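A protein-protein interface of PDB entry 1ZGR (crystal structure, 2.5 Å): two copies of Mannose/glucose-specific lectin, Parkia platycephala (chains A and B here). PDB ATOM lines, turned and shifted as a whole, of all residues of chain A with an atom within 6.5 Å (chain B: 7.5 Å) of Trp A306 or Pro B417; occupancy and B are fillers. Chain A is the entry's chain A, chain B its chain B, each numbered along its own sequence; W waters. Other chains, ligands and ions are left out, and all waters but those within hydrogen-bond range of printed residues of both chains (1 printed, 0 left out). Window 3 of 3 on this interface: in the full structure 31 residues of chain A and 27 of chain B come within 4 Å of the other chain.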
ATOM      1  N   SER A 302      -3.976   8.567  29.321  1.00  0.00           N
ATOM      2  CA  SER A 302      -2.913   7.775  28.739  1.00  0.00           C
ATOM      3  C   SER A 302      -3.253   6.310  28.886  1.00  0.00           C
ATOM      4  O   SER A 302      -3.686   5.912  29.938  1.00  0.00           O
ATOM      5  CB  SER A 302      -1.610   8.066  29.482  1.00  0.00           C
ATOM      6  OG  SER A 302      -0.643   7.088  29.178  1.00  0.00           O
ATOM      7  N   ILE A 303      -3.041   5.512  27.838  1.00  0.00           N
ATOM      8  CA  ILE A 303      -3.273   4.055  27.878  1.00  0.00           C
ATOM      9  C   ILE A 303      -2.043   3.247  27.369  1.00  0.00           C
ATOM     10  O   ILE A 303      -1.376   3.636  26.402  1.00  0.00           O
ATOM     11  CB  ILE A 303      -4.533   3.686  27.082  1.00  0.00           C
ATOM     12  CG1 ILE A 303      -5.675   4.655  27.405  1.00  0.00           C
ATOM     13  CG2 ILE A 303      -4.984   2.258  27.410  1.00  0.00           C
ATOM     14  CD1 ILE A 303      -7.034   4.218  26.929  1.00  0.00           C
ATOM     15  N   GLY A 304      -1.740   2.131  28.020  1.00  0.00           N
ATOM     16  CA  GLY A 304      -0.516   1.387  27.722  1.00  0.00           C
ATOM     17  C   GLY A 304       0.626   2.027  28.464  1.00  0.00           C
ATOM     18  O   GLY A 304       0.371   2.690  29.457  1.00  0.00           O
ATOM     19  N   PRO A 305       1.873   1.882  28.004  1.00  0.00           N
ATOM     20  CA  PRO A 305       2.210   1.156  26.755  1.00  0.00           C
ATOM     21  C   PRO A 305       2.070  -0.340  26.865  1.00  0.00           C
ATOM     22  O   PRO A 305       1.920  -0.870  27.977  1.00  0.00           O
ATOM     23  CB  PRO A 305       3.672   1.525  26.484  1.00  0.00           C
ATOM     24  CG  PRO A 305       4.203   2.318  27.746  1.00  0.00           C
ATOM     25  CD  PRO A 305       3.053   2.442  28.693  1.00  0.00           C
ATOM     26  N   TRP A 306       2.066  -1.016  25.713  1.00  0.00           N
ATOM     27  CA  TRP A 306       2.147  -2.477  25.661  1.00  0.00           C
ATOM     28  C   TRP A 306       3.496  -2.778  25.107  1.00  0.00           C
ATOM     29  O   TRP A 306       4.050  -1.957  24.406  1.00  0.00           O
ATOM     30  CB  TRP A 306       1.054  -3.087  24.745  1.00  0.00           C
ATOM     31  CG  TRP A 306      -0.318  -2.893  25.290  1.00  0.00           C
ATOM     32  CD1 TRP A 306      -0.959  -3.693  26.189  1.00  0.00           C
ATOM     33  CD2 TRP A 306      -1.213  -1.804  25.008  1.00  0.00           C
ATOM     34  NE1 TRP A 306      -2.196  -3.173  26.477  1.00  0.00           N
ATOM     35  CE2 TRP A 306      -2.376  -2.012  25.769  1.00  0.00           C
ATOM     36  CE3 TRP A 306      -1.158  -0.689  24.165  1.00  0.00           C
ATOM     37  CZ2 TRP A 306      -3.477  -1.146  25.722  1.00  0.00           C
ATOM     38  CZ3 TRP A 306      -2.244   0.183  24.133  1.00  0.00           C
ATOM     39  CH2 TRP A 306      -3.386  -0.056  24.910  1.00  0.00           C
ATOM     40  N   GLY A 307       4.033  -3.959  25.372  1.00  0.00           N
ATOM     41  CA  GLY A 307       5.342  -4.335  24.818  1.00  0.00           C
ATOM     42  C   GLY A 307       6.384  -4.530  25.909  1.00  0.00           C
ATOM     43  O   GLY A 307       6.033  -4.675  27.083  1.00  0.00           O
ATOM     44  N   GLY A 308       7.660  -4.521  25.521  1.00  0.00           N
ATOM     45  CA  GLY A 308       8.754  -4.755  26.457  1.00  0.00           C
ATOM     46  C   GLY A 308       9.189  -3.547  27.250  1.00  0.00           C
ATOM     47  O   GLY A 308       8.695  -2.424  27.029  1.00  0.00           O
ATOM     48  N   ILE A 375      -5.238   1.522  18.585  1.00  0.00           N
ATOM     49  CA  ILE A 375      -4.192   0.704  18.013  1.00  0.00           C
ATOM     50  C   ILE A 375      -4.417  -0.673  18.554  1.00  0.00           C
ATOM     51  O   ILE A 375      -5.124  -0.865  19.551  1.00  0.00           O
ATOM     52  CB  ILE A 375      -2.744   1.211  18.403  1.00  0.00           C
ATOM     53  CG1 ILE A 375      -2.560   1.185  19.921  1.00  0.00           C
ATOM     54  CG2 ILE A 375      -2.469   2.615  17.843  1.00  0.00           C
ATOM     55  CD1 ILE A 375      -1.188   1.292  20.330  1.00  0.00           C
ATOM     56  N   TYR A 379       3.113  -8.297  20.725  1.00  0.00           N
ATOM     57  CA  TYR A 379       4.502  -8.217  21.095  1.00  0.00           C
ATOM     58  C   TYR A 379       5.092  -9.567  21.503  1.00  0.00           C
ATOM     59  O   TYR A 379       4.358 -10.469  21.956  1.00  0.00           O
ATOM     60  CB  TYR A 379       4.695  -7.191  22.205  1.00  0.00           C
ATOM     61  CG  TYR A 379       3.908  -7.453  23.458  1.00  0.00           C
ATOM     62  CD1 TYR A 379       4.433  -8.251  24.491  1.00  0.00           C
ATOM     63  CD2 TYR A 379       2.663  -6.867  23.645  1.00  0.00           C
ATOM     64  CE1 TYR A 379       3.720  -8.468  25.671  1.00  0.00           C
ATOM     65  CE2 TYR A 379       1.941  -7.083  24.814  1.00  0.00           C
ATOM     66  CZ  TYR A 379       2.481  -7.881  25.814  1.00  0.00           C
ATOM     67  OH  TYR A 379       1.762  -8.085  26.948  1.00  0.00           O
ATOM     68  N   ILE A 391       7.461  -4.702  20.170  1.00  0.00           N
ATOM     69  CA  ILE A 391       6.273  -4.705  19.345  1.00  0.00           C
ATOM     70  C   ILE A 391       6.601  -5.531  18.093  1.00  0.00           C
ATOM     71  O   ILE A 391       7.546  -5.213  17.385  1.00  0.00           O
ATOM     72  CB  ILE A 391       5.886  -3.248  18.981  1.00  0.00           C
ATOM     73  CG1 ILE A 391       5.597  -2.400  20.242  1.00  0.00           C
ATOM     74  CG2 ILE A 391       4.709  -3.202  18.008  1.00  0.00           C
ATOM     75  CD1 ILE A 391       4.418  -2.879  21.101  1.00  0.00           C
ATOM     76  N   SER A 413      -1.202 -10.853  22.034  1.00  0.00           N
ATOM     77  CA  SER A 413      -1.833  -9.798  21.317  1.00  0.00           C
ATOM     78  C   SER A 413      -2.269  -8.714  22.285  1.00  0.00           C
ATOM     79  O   SER A 413      -2.359  -8.940  23.500  1.00  0.00           O
ATOM     80  CB  SER A 413      -3.005 -10.354  20.520  1.00  0.00           C
ATOM     81  OG  SER A 413      -3.998 -10.744  21.419  1.00  0.00           O
ATOM     82  N   PHE A 414      -2.494  -7.513  21.769  1.00  0.00           N
ATOM     83  CA  PHE A 414      -3.018  -6.446  22.609  1.00  0.00           C
ATOM     84  C   PHE A 414      -4.019  -5.630  21.809  1.00  0.00           C
ATOM     85  O   PHE A 414      -3.935  -5.578  20.567  1.00  0.00           O
ATOM     86  CB  PHE A 414      -1.884  -5.586  23.199  1.00  0.00           C
ATOM     87  CG  PHE A 414      -1.104  -4.781  22.180  1.00  0.00           C
ATOM     88  CD1 PHE A 414      -1.499  -3.504  21.843  1.00  0.00           C
ATOM     89  CD2 PHE A 414       0.053  -5.287  21.607  1.00  0.00           C
ATOM     90  CE1 PHE A 414      -0.779  -2.747  20.937  1.00  0.00           C
ATOM     91  CE2 PHE A 414       0.786  -4.541  20.691  1.00  0.00           C
ATOM     92  CZ  PHE A 414       0.369  -3.267  20.352  1.00  0.00           C
ATOM     93  N   SER A 415      -4.971  -5.012  22.512  1.00  0.00           N
ATOM     94  CA  SER A 415      -6.037  -4.222  21.884  1.00  0.00           C
ATOM     95  C   SER A 415      -6.829  -3.497  22.966  1.00  0.00           C
ATOM     96  O   SER A 415      -6.735  -3.884  24.129  1.00  0.00           O
ATOM     97  CB  SER A 415      -6.972  -5.105  21.070  1.00  0.00           C
ATOM     98  OG  SER A 415      -7.819  -5.829  21.944  1.00  0.00           O
ATOM     99  N   ILE A 416      -7.601  -2.471  22.583  1.00  0.00           N
ATOM    100  CA  ILE A 416      -8.300  -1.576  23.521  1.00  0.00           C
ATOM    101  C   ILE A 416      -9.753  -1.439  23.058  1.00  0.00           C
ATOM    102  O   ILE A 416     -10.007  -0.704  22.108  1.00  0.00           O
ATOM    103  CB  ILE A 416      -7.687  -0.124  23.471  1.00  0.00           C
ATOM    104  CG1 ILE A 416      -6.236  -0.115  23.007  1.00  0.00           C
ATOM    105  CG2 ILE A 416      -7.921   0.664  24.769  1.00  0.00           C
ATOM    106  CD1 ILE A 416      -5.914   1.118  22.226  1.00  0.00           C
ATOM    107  N   ARG A 429       8.522   3.084  24.427  1.00  0.00           N
ATOM    108  CA  ARG A 429       9.974   2.987  24.466  1.00  0.00           C
ATOM    109  C   ARG A 429      10.430   2.524  23.114  1.00  0.00           C
ATOM    110  O   ARG A 429       9.703   1.787  22.433  1.00  0.00           O
ATOM    111  CB  ARG A 429      10.447   2.038  25.578  1.00  0.00           C
ATOM    112  CG  ARG A 429      10.108   2.577  26.964  1.00  0.00           C
ATOM    113  CD  ARG A 429      10.296   1.602  28.100  1.00  0.00           C
ATOM    114  NE  ARG A 429       9.388   0.464  28.034  1.00  0.00           N
ATOM    115  CZ  ARG A 429       8.180   0.445  28.589  1.00  0.00           C
ATOM    116  NH1 ARG A 429       7.738   1.507  29.234  1.00  0.00           N
ATOM    117  NH2 ARG A 429       7.405  -0.629  28.480  1.00  0.00           N
ATOM    118  N   ASP A 435      10.191  -1.111  21.245  1.00  0.00           N
ATOM    119  CA  ASP A 435       9.923  -1.993  22.406  1.00  0.00           C
ATOM    120  C   ASP A 435       8.475  -1.946  22.892  1.00  0.00           C
ATOM    121  O   ASP A 435       7.898  -2.986  23.255  1.00  0.00           O
ATOM    122  CB  ASP A 435      10.838  -1.610  23.575  1.00  0.00           C
ATOM    123  CG  ASP A 435      12.305  -1.575  23.182  1.00  0.00           C
ATOM    124  OD1 ASP A 435      13.062  -2.440  23.681  1.00  0.00           O
ATOM    125  OD2 ASP A 435      12.786  -0.742  22.372  1.00  0.00           O
ATOM    126  N   ALA A 436       7.887  -0.746  22.934  1.00  0.00           N
ATOM    127  CA  ALA A 436       6.576  -0.581  23.535  1.00  0.00           C
ATOM    128  C   ALA A 436       5.875   0.649  22.976  1.00  0.00           C
ATOM    129  O   ALA A 436       6.541   1.615  22.594  1.00  0.00           O
ATOM    130  CB  ALA A 436       6.708  -0.464  25.070  1.00  0.00           C
ATOM    131  N   ILE A 437       4.539   0.605  22.921  1.00  0.00           N
ATOM    132  CA  ILE A 437       3.742   1.741  22.415  1.00  0.00           C
ATOM    133  C   ILE A 437       2.378   1.839  23.085  1.00  0.00           C
ATOM    134  O   ILE A 437       1.744   0.816  23.379  1.00  0.00           O
ATOM    135  CB  ILE A 437       3.582   1.722  20.874  1.00  0.00           C
ATOM    136  CG1 ILE A 437       2.988   3.067  20.392  1.00  0.00           C
ATOM    137  CG2 ILE A 437       2.721   0.534  20.420  1.00  0.00           C
ATOM    138  CD1 ILE A 437       3.221   3.374  18.896  1.00  0.00           C
ATOM    139  N   GLY A 438       1.941   3.076  23.330  1.00  0.00           N
ATOM    140  CA  GLY A 438       0.588   3.330  23.854  1.00  0.00           C
ATOM    141  C   GLY A 438       0.034   4.642  23.322  1.00  0.00           C
ATOM    142  O   GLY A 438       0.677   5.286  22.476  1.00  0.00           O
ATOM    143  N   ILE A 439      -1.121   5.073  23.828  1.00  0.00           N
ATOM    144  CA  ILE A 439      -1.790   6.254  23.246  1.00  0.00           C
ATOM    145  C   ILE A 439      -2.208   7.316  24.269  1.00  0.00           C
ATOM    146  O   ILE A 439      -2.378   7.026  25.449  1.00  0.00           O
ATOM    147  CB  ILE A 439      -3.018   5.799  22.389  1.00  0.00           C
ATOM    148  CG1 ILE A 439      -3.934   4.912  23.228  1.00  0.00           C
ATOM    149  CG2 ILE A 439      -2.540   5.016  21.119  1.00  0.00           C
ATOM    150  CD1 ILE A 439      -5.231   4.475  22.540  1.00  0.00           C
ATOM    151  N   TRP B 306     -15.834  -6.350  28.938  1.00  0.00           N
ATOM    152  CA  TRP B 306     -15.142  -7.627  28.801  1.00  0.00           C
ATOM    153  C   TRP B 306     -16.052  -8.658  29.395  1.00  0.00           C
ATOM    154  O   TRP B 306     -16.764  -8.364  30.363  1.00  0.00           O
ATOM    155  CB  TRP B 306     -13.818  -7.644  29.592  1.00  0.00           C
ATOM    156  CG  TRP B 306     -12.823  -6.649  29.122  1.00  0.00           C
ATOM    157  CD1 TRP B 306     -11.955  -6.799  28.092  1.00  0.00           C
ATOM    158  CD2 TRP B 306     -12.602  -5.337  29.651  1.00  0.00           C
ATOM    159  NE1 TRP B 306     -11.202  -5.658  27.942  1.00  0.00           N
ATOM    160  CE2 TRP B 306     -11.576  -4.745  28.889  1.00  0.00           C
ATOM    161  CE3 TRP B 306     -13.169  -4.600  30.699  1.00  0.00           C
ATOM    162  CZ2 TRP B 306     -11.101  -3.453  29.132  1.00  0.00           C
ATOM    163  CZ3 TRP B 306     -12.696  -3.311  30.946  1.00  0.00           C
ATOM    164  CH2 TRP B 306     -11.673  -2.755  30.162  1.00  0.00           C
ATOM    165  N   SER B 374      -9.919   2.086  37.693  1.00  0.00           N
ATOM    166  CA  SER B 374     -10.005   1.113  36.629  1.00  0.00           C
ATOM    167  C   SER B 374     -10.628  -0.130  37.205  1.00  0.00           C
ATOM    168  O   SER B 374     -11.110  -0.107  38.327  1.00  0.00           O
ATOM    169  CB  SER B 374      -8.622   0.740  36.176  1.00  0.00           C
ATOM    170  OG  SER B 374      -8.027   0.073  37.277  1.00  0.00           O
ATOM    171  N   ILE B 375     -10.630  -1.199  36.411  1.00  0.00           N
ATOM    172  CA  ILE B 375     -11.048  -2.509  36.854  1.00  0.00           C
ATOM    173  C   ILE B 375     -10.159  -3.558  36.202  1.00  0.00           C
ATOM    174  O   ILE B 375      -9.414  -3.268  35.235  1.00  0.00           O
ATOM    175  CB  ILE B 375     -12.540  -2.804  36.507  1.00  0.00           C
ATOM    176  CG1 ILE B 375     -12.801  -2.626  35.005  1.00  0.00           C
ATOM    177  CG2 ILE B 375     -13.519  -2.000  37.406  1.00  0.00           C
ATOM    178  CD1 ILE B 375     -14.141  -3.148  34.555  1.00  0.00           C
ATOM    179  N   SER B 415      -7.406  -6.616  31.981  1.00  0.00           N
ATOM    180  CA  SER B 415      -7.086  -5.367  32.721  1.00  0.00           C
ATOM    181  C   SER B 415      -6.919  -4.171  31.762  1.00  0.00           C
ATOM    182  O   SER B 415      -6.862  -4.337  30.537  1.00  0.00           O
ATOM    183  CB  SER B 415      -5.829  -5.524  33.596  1.00  0.00           C
ATOM    184  OG  SER B 415      -4.679  -5.813  32.808  1.00  0.00           O
ATOM    185  N   ILE B 416      -6.850  -2.967  32.337  1.00  0.00           N
ATOM    186  CA  ILE B 416      -6.717  -1.708  31.589  1.00  0.00           C
ATOM    187  C   ILE B 416      -5.505  -0.953  32.102  1.00  0.00           C
ATOM    188  O   ILE B 416      -5.510  -0.474  33.228  1.00  0.00           O
ATOM    189  CB  ILE B 416      -7.941  -0.790  31.805  1.00  0.00           C
ATOM    190  CG1 ILE B 416      -9.230  -1.600  31.870  1.00  0.00           C
ATOM    191  CG2 ILE B 416      -7.989   0.295  30.729  1.00  0.00           C
ATOM    192  CD1 ILE B 416     -10.367  -0.915  32.646  1.00  0.00           C
ATOM    193  N   PRO B 417      -4.480  -0.844  31.270  1.00  0.00           N
ATOM    194  CA  PRO B 417      -3.312  -0.037  31.590  1.00  0.00           C
ATOM    195  C   PRO B 417      -3.550   1.441  31.306  1.00  0.00           C
ATOM    196  O   PRO B 417      -2.976   1.977  30.382  1.00  0.00           O
ATOM    197  CB  PRO B 417      -2.215  -0.615  30.683  1.00  0.00           C
ATOM    198  CG  PRO B 417      -2.948  -1.217  29.498  1.00  0.00           C
ATOM    199  CD  PRO B 417      -4.362  -1.535  29.966  1.00  0.00           C
ATOM    200  N   ILE B 418      -4.368   2.090  32.133  1.00  0.00           N
ATOM    201  CA  ILE B 418      -4.810   3.479  31.960  1.00  0.00           C
ATOM    202  C   ILE B 418      -4.343   4.376  33.110  1.00  0.00           C
ATOM    203  O   ILE B 418      -4.284   3.935  34.253  1.00  0.00           O
ATOM    204  CB  ILE B 418      -6.366   3.488  31.860  1.00  0.00           C
ATOM    205  CG1 ILE B 418      -6.898   4.841  31.427  1.00  0.00           C
ATOM    206  CG2 ILE B 418      -7.025   3.061  33.183  1.00  0.00           C
ATOM    207  CD1 ILE B 418      -8.396   4.856  31.307  1.00  0.00           C
ATOM    208  N   HIS B 419      -4.027   5.636  32.807  1.00  0.00           N
ATOM    209  CA  HIS B 419      -3.603   6.624  33.805  1.00  0.00           C
ATOM    210  C   HIS B 419      -4.197   7.984  33.492  1.00  0.00           C
ATOM    211  O   HIS B 419      -4.714   8.216  32.367  1.00  0.00           O
ATOM    212  CB  HIS B 419      -2.076   6.780  33.832  1.00  0.00           C
ATOM    213  CG  HIS B 419      -1.337   5.491  34.033  1.00  0.00           C
ATOM    214  ND1 HIS B 419      -0.894   5.068  35.272  1.00  0.00           N
ATOM    215  CD2 HIS B 419      -0.986   4.521  33.150  1.00  0.00           C
ATOM    216  CE1 HIS B 419      -0.292   3.898  35.139  1.00  0.00           C
ATOM    217  NE2 HIS B 419      -0.341   3.542  33.864  1.00  0.00           N
ATOM    218  N   ASN B 421      -6.842   9.294  34.622  1.00  0.00           N
ATOM    219  CA  ASN B 421      -8.298   9.222  34.417  1.00  0.00           C
ATOM    220  C   ASN B 421      -9.093   9.018  35.710  1.00  0.00           C
ATOM    221  O   ASN B 421      -8.573   8.535  36.712  1.00  0.00           O
ATOM    222  CB  ASN B 421      -8.634   8.047  33.498  1.00  0.00           C
ATOM    223  CG  ASN B 421      -8.441   6.725  34.192  1.00  0.00           C
ATOM    224  OD1 ASN B 421      -7.331   6.397  34.570  1.00  0.00           O
ATOM    225  ND2 ASN B 421      -9.524   5.974  34.393  1.00  0.00           N
HETATM  226  O   HOH W   1      -8.477  -5.367  26.504  1.00  0.00           O
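Positions printed for both chains: 306, 375, 415 and 416.
The backbone NH of Ile A303 lies within hydrogen-bond range of the backbone carbonyl oxygen of Ile A439, at 2.9 Å.
The backbone NH (N) of Trp A306 is in hydrogen-bond range of the backbone carbonyl oxygen (O) of Ile A437.
Water W1 lies within hydrogen-bond range of NE1 of Trp B306 (3.1 Å) and O of Ser A415 (3.3 Å).
Pro B417 touches just these residues of chain A: Ile A303 (3.3 Å), Gly A304 (2.7 Å) and Trp A306 (3.7 Å).
Of the printed residues of chain B, Gly A304 touches Pro B417 (2.7 Å).
Of the printed residues of chain A, Ile B418 touches Ser A302.
Of the printed residues of chain A, His B419 touches Ser A302.
Of the printed residues of chain B, Ser A302 touches Ile B418 (3.4 Å) and His B419 (2.9 Å).
Of the printed residues of chain B, Ile A303 touches Pro B417 (3.3 Å).
The nearest residue of chain B that does not touch Trp A306 is Ser B415 (6.3 Å).
The nearest residue of chain A that does not touch Pro B417 is Ser A302 (4.02 Å).
The backbone carbonyl oxygen (O) of Ser A302 lies within hydrogen-bond range of the backbone NH (N) of His B419.
O of Pro B417 sits at hydrogen-bond distance from N of Gly A304 (2.7 Å).
O of Ser A302 touches CA of Ile B418, at 3.4 Å.
O of Pro B417 touches CA of Ile A303, 3.3 Å away.
NE1 of Trp A306 touches CG of Pro B417, 3.7 Å away.
Of the 20 printed residues of chain A, 4 touch a printed residue of chain B.
Hydrophobic or aromatic side chains of chain A that line the printed part of chain B: Ile A303 and Trp A306.
Printed residues of chain B that touch a printed residue of chain A: Pro B417, Ile B418 and His B419.
Hydrophobic or aromatic side chains of chain B within 4 Å of the printed part of chain A: Pro B417 and Ile B418.
Among the printed residues, no Asp or Glu carboxylate lies within 4 Å of a Lys or Arg side-chain nitrogen of the other chain.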
